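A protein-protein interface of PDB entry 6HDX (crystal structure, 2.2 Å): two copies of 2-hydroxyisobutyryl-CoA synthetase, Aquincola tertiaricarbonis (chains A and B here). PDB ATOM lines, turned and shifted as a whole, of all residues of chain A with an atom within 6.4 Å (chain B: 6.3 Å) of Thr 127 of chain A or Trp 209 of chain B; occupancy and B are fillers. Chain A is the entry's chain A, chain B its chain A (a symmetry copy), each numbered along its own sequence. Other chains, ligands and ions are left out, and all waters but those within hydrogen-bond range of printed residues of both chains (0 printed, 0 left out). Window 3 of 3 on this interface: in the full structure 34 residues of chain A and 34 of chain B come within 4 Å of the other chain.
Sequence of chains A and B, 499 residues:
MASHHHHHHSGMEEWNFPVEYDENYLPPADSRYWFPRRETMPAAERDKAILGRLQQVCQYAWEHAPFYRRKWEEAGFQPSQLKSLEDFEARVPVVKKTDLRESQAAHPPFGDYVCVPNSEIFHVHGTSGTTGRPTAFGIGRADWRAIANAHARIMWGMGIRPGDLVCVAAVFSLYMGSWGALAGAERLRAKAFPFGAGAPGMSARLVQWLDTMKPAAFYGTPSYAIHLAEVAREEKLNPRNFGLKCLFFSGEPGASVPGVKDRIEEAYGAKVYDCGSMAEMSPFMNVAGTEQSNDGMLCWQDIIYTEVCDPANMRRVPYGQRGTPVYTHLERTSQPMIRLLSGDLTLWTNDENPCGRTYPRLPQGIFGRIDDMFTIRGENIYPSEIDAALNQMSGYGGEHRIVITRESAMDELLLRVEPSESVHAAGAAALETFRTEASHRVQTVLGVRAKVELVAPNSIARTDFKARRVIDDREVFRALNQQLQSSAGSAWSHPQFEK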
ATOM      1  N   ARG A 101      13.152  29.544  12.778  1.00  0.00           N
ATOM      2  CA  ARG A 101      13.533  28.329  12.059  1.00  0.00           C
ATOM      3  C   ARG A 101      14.946  28.441  11.502  1.00  0.00           C
ATOM      4  O   ARG A 101      15.762  27.572  11.804  1.00  0.00           O
ATOM      5  CB  ARG A 101      12.532  27.998  10.936  1.00  0.00           C
ATOM      6  CG  ARG A 101      11.195  27.504  11.427  1.00  0.00           C
ATOM      7  CD  ARG A 101      10.201  27.397  10.295  1.00  0.00           C
ATOM      8  NE  ARG A 101       8.836  27.442  10.812  1.00  0.00           N
ATOM      9  CZ  ARG A 101       7.865  28.180  10.291  1.00  0.00           C
ATOM     10  NH1 ARG A 101       8.094  28.928   9.219  1.00  0.00           N
ATOM     11  NH2 ARG A 101       6.650  28.157  10.823  1.00  0.00           N
ATOM     12  N   VAL A 124      12.499  20.261  27.235  1.00  0.00           N
ATOM     13  CA  VAL A 124      12.528  20.330  25.778  1.00  0.00           C
ATOM     14  C   VAL A 124      11.121  20.019  25.248  1.00  0.00           C
ATOM     15  O   VAL A 124      10.534  18.994  25.590  1.00  0.00           O
ATOM     16  CB  VAL A 124      13.636  19.466  25.102  1.00  0.00           C
ATOM     17  CG1 VAL A 124      13.606  19.629  23.581  1.00  0.00           C
ATOM     18  CG2 VAL A 124      15.022  19.826  25.645  1.00  0.00           C
ATOM     19  N   HIS A 125      10.556  20.960  24.478  1.00  0.00           N
ATOM     20  CA  HIS A 125       9.268  20.816  23.803  1.00  0.00           C
ATOM     21  C   HIS A 125       9.446  21.383  22.400  1.00  0.00           C
ATOM     22  O   HIS A 125      10.572  21.623  21.981  1.00  0.00           O
ATOM     23  CB  HIS A 125       8.150  21.553  24.574  1.00  0.00           C
ATOM     24  CG  HIS A 125       7.924  21.035  25.957  1.00  0.00           C
ATOM     25  ND1 HIS A 125       7.084  19.964  26.195  1.00  0.00           N
ATOM     26  CD2 HIS A 125       8.468  21.444  27.133  1.00  0.00           C
ATOM     27  CE1 HIS A 125       7.161  19.738  27.498  1.00  0.00           C
ATOM     28  NE2 HIS A 125       7.954  20.621  28.110  1.00  0.00           N
ATOM     29  N   GLY A 126       8.360  21.637  21.703  1.00  0.00           N
ATOM     30  CA  GLY A 126       8.444  22.218  20.373  1.00  0.00           C
ATOM     31  C   GLY A 126       7.131  22.306  19.631  1.00  0.00           C
ATOM     32  O   GLY A 126       6.058  22.152  20.215  1.00  0.00           O
ATOM     33  N   THR A 127       7.230  22.517  18.325  1.00  0.00           N
ATOM     34  CA  THR A 127       6.099  22.567  17.383  1.00  0.00           C
ATOM     35  C   THR A 127       6.112  21.287  16.504  1.00  0.00           C
ATOM     36  O   THR A 127       7.157  20.625  16.384  1.00  0.00           O
ATOM     37  CB  THR A 127       6.211  23.832  16.498  1.00  0.00           C
ATOM     38  OG1 THR A 127       7.349  23.682  15.651  1.00  0.00           O
ATOM     39  CG2 THR A 127       6.356  25.109  17.306  1.00  0.00           C
ATOM     40  N   SER A 128       4.968  20.962  15.863  1.00  0.00           N
ATOM     41  CA  SER A 128       4.817  19.809  14.957  1.00  0.00           C
ATOM     42  C   SER A 128       3.816  20.106  13.838  1.00  0.00           C
ATOM     43  O   SER A 128       2.956  20.976  13.988  1.00  0.00           O
ATOM     44  CB  SER A 128       4.408  18.553  15.725  1.00  0.00           C
ATOM     45  OG  SER A 128       3.108  18.644  16.289  1.00  0.00           O
ATOM     46  N   ARG A 133       9.322  23.422   8.816  1.00  0.00           N
ATOM     47  CA  ARG A 133      10.273  22.881   9.788  1.00  0.00           C
ATOM     48  C   ARG A 133       9.834  23.161  11.237  1.00  0.00           C
ATOM     49  O   ARG A 133       9.364  24.269  11.546  1.00  0.00           O
ATOM     50  CB  ARG A 133      11.704  23.391   9.526  1.00  0.00           C
ATOM     51  CG  ARG A 133      12.777  22.292   9.524  1.00  0.00           C
ATOM     52  CD  ARG A 133      12.760  21.445   8.255  1.00  0.00           C
ATOM     53  NE  ARG A 133      13.854  20.471   8.219  1.00  0.00           N
ATOM     54  CZ  ARG A 133      14.116  19.668   7.189  1.00  0.00           C
ATOM     55  NH1 ARG A 133      15.134  18.819   7.243  1.00  0.00           N
ATOM     56  NH2 ARG A 133      13.363  19.710   6.095  1.00  0.00           N
ATOM     57  N   PRO A 134       9.925  22.149  12.138  1.00  0.00           N
ATOM     58  CA  PRO A 134       9.496  22.385  13.524  1.00  0.00           C
ATOM     59  C   PRO A 134      10.585  23.071  14.362  1.00  0.00           C
ATOM     60  O   PRO A 134      11.770  22.897  14.097  1.00  0.00           O
ATOM     61  CB  PRO A 134       9.172  20.978  14.026  1.00  0.00           C
ATOM     62  CG  PRO A 134      10.051  20.072  13.238  1.00  0.00           C
ATOM     63  CD  PRO A 134      10.439  20.768  11.958  1.00  0.00           C
ATOM     64  N   THR A 135      10.185  23.840  15.374  1.00  0.00           N
ATOM     65  CA  THR A 135      11.168  24.483  16.237  1.00  0.00           C
ATOM     66  C   THR A 135      11.170  23.849  17.594  1.00  0.00           C
ATOM     67  O   THR A 135      10.123  23.446  18.090  1.00  0.00           O
ATOM     68  CB  THR A 135      10.994  26.007  16.306  1.00  0.00           C
ATOM     69  OG1 THR A 135       9.661  26.303  16.695  1.00  0.00           O
ATOM     70  CG2 THR A 135      11.350  26.693  15.000  1.00  0.00           C
ATOM     71  N   ALA A 136      12.349  23.753  18.186  1.00  0.00           N
ATOM     72  CA  ALA A 136      12.546  23.213  19.517  1.00  0.00           C
ATOM     73  C   ALA A 136      12.515  24.326  20.559  1.00  0.00           C
ATOM     74  O   ALA A 136      13.148  25.366  20.389  1.00  0.00           O
ATOM     75  CB  ALA A 136      13.892  22.505  19.583  1.00  0.00           C
ATOM     76  N   PHE A 137      11.820  24.079  21.658  1.00  0.00           N
ATOM     77  CA  PHE A 137      11.795  24.964  22.800  1.00  0.00           C
ATOM     78  C   PHE A 137      12.730  24.372  23.851  1.00  0.00           C
ATOM     79  O   PHE A 137      12.611  23.202  24.207  1.00  0.00           O
ATOM     80  CB  PHE A 137      10.368  25.159  23.337  1.00  0.00           C
ATOM     81  CG  PHE A 137       9.390  25.681  22.298  1.00  0.00           C
ATOM     82  CD1 PHE A 137       9.741  26.730  21.446  1.00  0.00           C
ATOM     83  CD2 PHE A 137       8.103  25.167  22.212  1.00  0.00           C
ATOM     84  CE1 PHE A 137       8.828  27.227  20.509  1.00  0.00           C
ATOM     85  CE2 PHE A 137       7.203  25.650  21.257  1.00  0.00           C
ATOM     86  CZ  PHE A 137       7.562  26.683  20.425  1.00  0.00           C
ATOM     87  N   LEU A 174       5.183  17.387  22.666  1.00  0.00           N
ATOM     88  CA  LEU A 174       5.857  18.624  22.235  1.00  0.00           C
ATOM     89  C   LEU A 174       5.015  19.861  22.570  1.00  0.00           C
ATOM     90  O   LEU A 174       5.561  20.903  22.901  1.00  0.00           O
ATOM     91  CB  LEU A 174       6.076  18.567  20.707  1.00  0.00           C
ATOM     92  CG  LEU A 174       7.148  17.606  20.179  1.00  0.00           C
ATOM     93  CD1 LEU A 174       7.096  17.558  18.697  1.00  0.00           C
ATOM     94  CD2 LEU A 174       8.555  18.026  20.629  1.00  0.00           C
ATOM     95  N   TYR A 175       3.691  19.734  22.476  1.00  0.00           N
ATOM     96  CA  TYR A 175       2.682  20.783  22.667  1.00  0.00           C
ATOM     97  C   TYR A 175       2.725  21.457  24.049  1.00  0.00           C
ATOM     98  O   TYR A 175       2.605  20.781  25.077  1.00  0.00           O
ATOM     99  CB  TYR A 175       1.301  20.196  22.358  1.00  0.00           C
ATOM    100  CG  TYR A 175       0.167  21.190  22.467  1.00  0.00           C
ATOM    101  CD1 TYR A 175       0.122  22.321  21.651  1.00  0.00           C
ATOM    102  CD2 TYR A 175      -0.892  20.975  23.344  1.00  0.00           C
ATOM    103  CE1 TYR A 175      -0.945  23.216  21.713  1.00  0.00           C
ATOM    104  CE2 TYR A 175      -1.970  21.855  23.405  1.00  0.00           C
ATOM    105  CZ  TYR A 175      -1.988  22.978  22.592  1.00  0.00           C
ATOM    106  OH  TYR A 175      -3.037  23.849  22.640  1.00  0.00           O
ATOM    107  N   ALA A 279       2.693  29.054  21.680  1.00  0.00           N
ATOM    108  CA  ALA A 279       3.619  28.169  22.395  1.00  0.00           C
ATOM    109  C   ALA A 279       4.949  28.867  22.623  1.00  0.00           C
ATOM    110  O   ALA A 279       5.548  28.705  23.690  1.00  0.00           O
ATOM    111  CB  ALA A 279       3.833  26.893  21.581  1.00  0.00           C
ATOM    112  N   GLU A 280       5.415  29.655  21.624  1.00  0.00           N
ATOM    113  CA  GLU A 280       6.668  30.433  21.709  1.00  0.00           C
ATOM    114  C   GLU A 280       6.548  31.468  22.835  1.00  0.00           C
ATOM    115  O   GLU A 280       7.551  31.858  23.449  1.00  0.00           O
ATOM    116  CB  GLU A 280       6.958  31.190  20.394  1.00  0.00           C
ATOM    117  CG  GLU A 280       7.268  30.326  19.188  1.00  0.00           C
ATOM    118  CD  GLU A 280       6.064  29.732  18.468  1.00  0.00           C
ATOM    119  OE1 GLU A 280       4.909  29.948  18.904  1.00  0.00           O
ATOM    120  OE2 GLU A 280       6.287  29.021  17.468  1.00  0.00           O
ATOM    121  N   LEU B 165      20.392  15.115  27.770  1.00  0.00           N
ATOM    122  CA  LEU B 165      19.077  15.138  27.175  1.00  0.00           C
ATOM    123  C   LEU B 165      18.437  13.750  27.393  1.00  0.00           C
ATOM    124  O   LEU B 165      18.973  12.736  26.924  1.00  0.00           O
ATOM    125  CB  LEU B 165      19.184  15.474  25.684  1.00  0.00           C
ATOM    126  CG  LEU B 165      17.826  15.658  24.970  1.00  0.00           C
ATOM    127  CD1 LEU B 165      17.171  16.937  25.392  1.00  0.00           C
ATOM    128  CD2 LEU B 165      18.003  15.671  23.475  1.00  0.00           C
ATOM    129  N   PHE B 193      13.129  15.779  28.205  1.00  0.00           N
ATOM    130  CA  PHE B 193      12.444  15.854  26.912  1.00  0.00           C
ATOM    131  C   PHE B 193      11.187  14.930  26.952  1.00  0.00           C
ATOM    132  O   PHE B 193      11.245  13.784  26.494  1.00  0.00           O
ATOM    133  CB  PHE B 193      13.441  15.512  25.779  1.00  0.00           C
ATOM    134  CG  PHE B 193      12.910  15.428  24.372  1.00  0.00           C
ATOM    135  CD1 PHE B 193      11.856  16.247  23.952  1.00  0.00           C
ATOM    136  CD2 PHE B 193      13.476  14.549  23.450  1.00  0.00           C
ATOM    137  CE1 PHE B 193      11.375  16.177  22.639  1.00  0.00           C
ATOM    138  CE2 PHE B 193      12.998  14.482  22.133  1.00  0.00           C
ATOM    139  CZ  PHE B 193      11.949  15.293  21.736  1.00  0.00           C
ATOM    140  N   PHE B 195       8.520  13.715  25.340  1.00  0.00           N
ATOM    141  CA  PHE B 195       7.848  13.524  24.056  1.00  0.00           C
ATOM    142  C   PHE B 195       6.578  12.705  24.253  1.00  0.00           C
ATOM    143  O   PHE B 195       5.612  12.950  23.569  1.00  0.00           O
ATOM    144  CB  PHE B 195       8.781  12.868  22.995  1.00  0.00           C
ATOM    145  CG  PHE B 195       8.202  12.848  21.587  1.00  0.00           C
ATOM    146  CD1 PHE B 195       7.400  11.786  21.158  1.00  0.00           C
ATOM    147  CD2 PHE B 195       8.468  13.881  20.691  1.00  0.00           C
ATOM    148  CE1 PHE B 195       6.855  11.772  19.871  1.00  0.00           C
ATOM    149  CE2 PHE B 195       7.886  13.886  19.415  1.00  0.00           C
ATOM    150  CZ  PHE B 195       7.081  12.829  19.013  1.00  0.00           C
ATOM    151  N   ALA B 204       6.812   8.261  14.027  1.00  0.00           N
ATOM    152  CA  ALA B 204       7.487   8.755  12.823  1.00  0.00           C
ATOM    153  C   ALA B 204       8.128  10.118  13.118  1.00  0.00           C
ATOM    154  O   ALA B 204       9.214  10.390  12.636  1.00  0.00           O
ATOM    155  CB  ALA B 204       6.501   8.855  11.663  1.00  0.00           C
ATOM    156  N   ARG B 205       7.471  10.952  13.946  1.00  0.00           N
ATOM    157  CA  ARG B 205       7.982  12.265  14.340  1.00  0.00           C
ATOM    158  C   ARG B 205       9.152  12.133  15.330  1.00  0.00           C
ATOM    159  O   ARG B 205      10.139  12.849  15.199  1.00  0.00           O
ATOM    160  CB  ARG B 205       6.859  13.097  14.946  1.00  0.00           C
ATOM    161  CG  ARG B 205       6.199  14.043  13.967  1.00  0.00           C
ATOM    162  CD  ARG B 205       4.870  14.595  14.501  1.00  0.00           C
ATOM    163  NE  ARG B 205       4.949  15.040  15.897  1.00  0.00           N
ATOM    164  CZ  ARG B 205       4.134  14.609  16.855  1.00  0.00           C
ATOM    165  NH1 ARG B 205       3.183  13.726  16.576  1.00  0.00           N
ATOM    166  NH2 ARG B 205       4.255  15.068  18.101  1.00  0.00           N
ATOM    167  N   LEU B 206       9.040  11.208  16.299  1.00  0.00           N
ATOM    168  CA  LEU B 206      10.058  10.949  17.323  1.00  0.00           C
ATOM    169  C   LEU B 206      11.430  10.593  16.752  1.00  0.00           C
ATOM    170  O   LEU B 206      12.418  11.149  17.205  1.00  0.00           O
ATOM    171  CB  LEU B 206       9.602   9.878  18.363  1.00  0.00           C
ATOM    172  CG  LEU B 206      10.580   9.623  19.557  1.00  0.00           C
ATOM    173  CD1 LEU B 206      10.986  10.956  20.262  1.00  0.00           C
ATOM    174  CD2 LEU B 206       9.986   8.632  20.554  1.00  0.00           C
ATOM    175  N   VAL B 207      11.500   9.676  15.787  1.00  0.00           N
ATOM    176  CA  VAL B 207      12.775   9.268  15.172  1.00  0.00           C
ATOM    177  C   VAL B 207      13.501  10.489  14.536  1.00  0.00           C
ATOM    178  O   VAL B 207      14.728  10.563  14.615  1.00  0.00           O
ATOM    179  CB  VAL B 207      12.648   8.039  14.212  1.00  0.00           C
ATOM    180  CG1 VAL B 207      12.169   6.812  14.983  1.00  0.00           C
ATOM    181  CG2 VAL B 207      11.716   8.318  13.031  1.00  0.00           C
ATOM    182  N   GLN B 208      12.747  11.454  13.970  1.00  0.00           N
ATOM    183  CA  GLN B 208      13.342  12.687  13.424  1.00  0.00           C
ATOM    184  C   GLN B 208      13.890  13.521  14.570  1.00  0.00           C
ATOM    185  O   GLN B 208      15.008  14.022  14.447  1.00  0.00           O
ATOM    186  CB  GLN B 208      12.324  13.523  12.609  1.00  0.00           C
ATOM    187  CG  GLN B 208      11.747  12.822  11.365  1.00  0.00           C
ATOM    188  CD  GLN B 208      12.762  12.562  10.243  1.00  0.00           C
ATOM    189  OE1 GLN B 208      13.883  13.108  10.200  1.00  0.00           O
ATOM    190  NE2 GLN B 208      12.377  11.715   9.297  1.00  0.00           N
ATOM    191  N   TRP B 209      13.129  13.633  15.713  1.00  0.00           N
ATOM    192  CA  TRP B 209      13.577  14.390  16.887  1.00  0.00           C
ATOM    193  C   TRP B 209      14.816  13.797  17.512  1.00  0.00           C
ATOM    194  O   TRP B 209      15.696  14.554  17.921  1.00  0.00           O
ATOM    195  CB  TRP B 209      12.470  14.558  17.934  1.00  0.00           C
ATOM    196  CG  TRP B 209      11.550  15.687  17.595  1.00  0.00           C
ATOM    197  CD1 TRP B 209      10.499  15.647  16.730  1.00  0.00           C
ATOM    198  CD2 TRP B 209      11.629  17.036  18.070  1.00  0.00           C
ATOM    199  NE1 TRP B 209       9.909  16.879  16.644  1.00  0.00           N
ATOM    200  CE2 TRP B 209      10.580  17.756  17.456  1.00  0.00           C
ATOM    201  CE3 TRP B 209      12.470  17.709  18.976  1.00  0.00           C
ATOM    202  CZ2 TRP B 209      10.362  19.120  17.696  1.00  0.00           C
ATOM    203  CZ3 TRP B 209      12.224  19.052  19.241  1.00  0.00           C
ATOM    204  CH2 TRP B 209      11.206  19.747  18.585  1.00  0.00           C
ATOM    205  N   LEU B 210      14.884  12.443  17.585  1.00  0.00           N
ATOM    206  CA  LEU B 210      16.028  11.701  18.118  1.00  0.00           C
ATOM    207  C   LEU B 210      17.251  11.890  17.208  1.00  0.00           C
ATOM    208  O   LEU B 210      18.351  12.099  17.716  1.00  0.00           O
ATOM    209  CB  LEU B 210      15.694  10.203  18.296  1.00  0.00           C
ATOM    210  CG  LEU B 210      14.523   9.841  19.246  1.00  0.00           C
ATOM    211  CD1 LEU B 210      14.303   8.361  19.281  1.00  0.00           C
ATOM    212  CD2 LEU B 210      14.733  10.364  20.653  1.00  0.00           C
ATOM    213  N   ASP B 211      17.052  11.869  15.867  1.00  0.00           N
ATOM    214  CA  ASP B 211      18.122  12.103  14.886  1.00  0.00           C
ATOM    215  C   ASP B 211      18.698  13.533  15.006  1.00  0.00           C
ATOM    216  O   ASP B 211      19.909  13.697  14.949  1.00  0.00           O
ATOM    217  CB  ASP B 211      17.627  11.825  13.448  1.00  0.00           C
ATOM    218  CG  ASP B 211      18.734  11.863  12.388  1.00  0.00           C
ATOM    219  OD1 ASP B 211      19.499  10.891  12.299  1.00  0.00           O
ATOM    220  OD2 ASP B 211      18.817  12.868  11.647  1.00  0.00           O
ATOM    221  N   THR B 212      17.835  14.553  15.203  1.00  0.00           N
ATOM    222  CA  THR B 212      18.247  15.960  15.359  1.00  0.00           C
ATOM    223  C   THR B 212      18.899  16.233  16.735  1.00  0.00           C
ATOM    224  O   THR B 212      20.024  16.730  16.787  1.00  0.00           O
ATOM    225  CB  THR B 212      17.038  16.883  15.114  1.00  0.00           C
ATOM    226  OG1 THR B 212      16.565  16.666  13.786  1.00  0.00           O
ATOM    227  CG2 THR B 212      17.359  18.375  15.328  1.00  0.00           C
ATOM    228  N   MET B 213      18.163  15.941  17.831  1.00  0.00           N
ATOM    229  CA  MET B 213      18.524  16.198  19.234  1.00  0.00           C
ATOM    230  C   MET B 213      19.629  15.318  19.782  1.00  0.00           C
ATOM    231  O   MET B 213      20.327  15.765  20.687  1.00  0.00           O
ATOM    232  CB  MET B 213      17.289  16.088  20.164  1.00  0.00           C
ATOM    233  CG  MET B 213      16.172  17.064  19.880  1.00  0.00           C
ATOM    234  SD  MET B 213      16.587  18.795  20.193  1.00  0.00           S
ATOM    235  CE  MET B 213      15.913  19.477  18.741  1.00  0.00           C
ATOM    236  N   LYS B 214      19.770  14.062  19.294  1.00  0.00           N
ATOM    237  CA  LYS B 214      20.811  13.103  19.755  1.00  0.00           C
ATOM    238  C   LYS B 214      20.800  12.935  21.312  1.00  0.00           C
ATOM    239  O   LYS B 214      21.754  13.350  21.969  1.00  0.00           O
ATOM    240  CB  LYS B 214      22.235  13.495  19.247  1.00  0.00           C
ATOM    241  CG  LYS B 214      22.336  13.839  17.767  1.00  0.00           C
ATOM    242  CD  LYS B 214      22.694  12.652  16.908  1.00  0.00           C
ATOM    243  CE  LYS B 214      23.115  13.085  15.526  1.00  0.00           C
ATOM    244  NZ  LYS B 214      22.388  12.310  14.484  1.00  0.00           N
ATOM    245  N   PRO B 215      19.739  12.373  21.938  1.00  0.00           N
ATOM    246  CA  PRO B 215      19.721  12.289  23.413  1.00  0.00           C
ATOM    247  C   PRO B 215      20.698  11.292  24.011  1.00  0.00           C
ATOM    248  O   PRO B 215      21.035  10.294  23.368  1.00  0.00           O
ATOM    249  CB  PRO B 215      18.272  11.882  23.716  1.00  0.00           C
ATOM    250  CG  PRO B 215      17.887  11.073  22.544  1.00  0.00           C
ATOM    251  CD  PRO B 215      18.493  11.816  21.372  1.00  0.00           C
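Among the printed residues, merely in contact across the chains: Val 124 of chain A with Leu 165 of chain B, Val 124 of chain A with Phe 193 of chain B, His 125 of chain A with Trp 209 of chain B, Thr 127 of chain A with Trp 209 of chain B, Ser 128 of chain A with Arg 205 of chain B, Thr 135 of chain A with Trp 209 of chain B, Ala 136 of chain A with Trp 209 of chain B, Ala 136 of chain A with Met 213 of chain B, Leu 174 of chain A with Phe 193 of chain B, Leu 174 of chain A with Phe 195 of chain B, Leu 174 of chain A with Arg 205 of chain B and Leu 174 of chain A with Trp 209 of chain B.
The backbone NH of Thr 135 of chain A sits at hydrogen-bond distance from the side-chain hydroxyl of Thr 127 of chain A (2.9 Å).
The backbone carbonyl oxygen (O) of Leu 174 of chain A sits at hydrogen-bond distance from the backbone NH (N) of Gly 126 of chain A (3.1 Å).
O of His 125 of chain A sits at hydrogen-bond distance from N of Phe 137 of chain A.
Of the printed residues of chain B, Val 124 of chain A touches Leu 165 (3.6 Å) and Phe 193 (3.5 Å).
Of the printed residues of chain B, His 125 of chain A touches Trp 209.
Ala 204 of chain B touches none of the printed residues of chain A.
Printed residues of chain A within 4 Å of Met 213 of chain B: Ala 136 (3.7 Å).
The nearest residue of chain A that does not touch Trp 209 of chain B is Gly 126 of chain A (4.1 Å).
No position is printed for both chains.
Of the 15 printed residues of chain B, 6 touch a printed residue of chain A.
Printed residues of chain B that touch a printed residue of chain A: Leu 165, Phe 193, Phe 195, Arg 205, Trp 209 and Met 213.
Hydrophobic or aromatic side chains of chain B within 4 Å of the printed part of chain A: Leu 165, Phe 193, Phe 195, Trp 209 and Met 213.
Along chain B the printed residues that touch a printed residue of chain A span positions 165 to 213.
Of the 15 printed residues of chain A, 7 touch a printed residue of chain B.
Hydrophobic or aromatic side chains of chain A that line the printed part of chain B: Val 124, Ala 136 and Leu 174.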
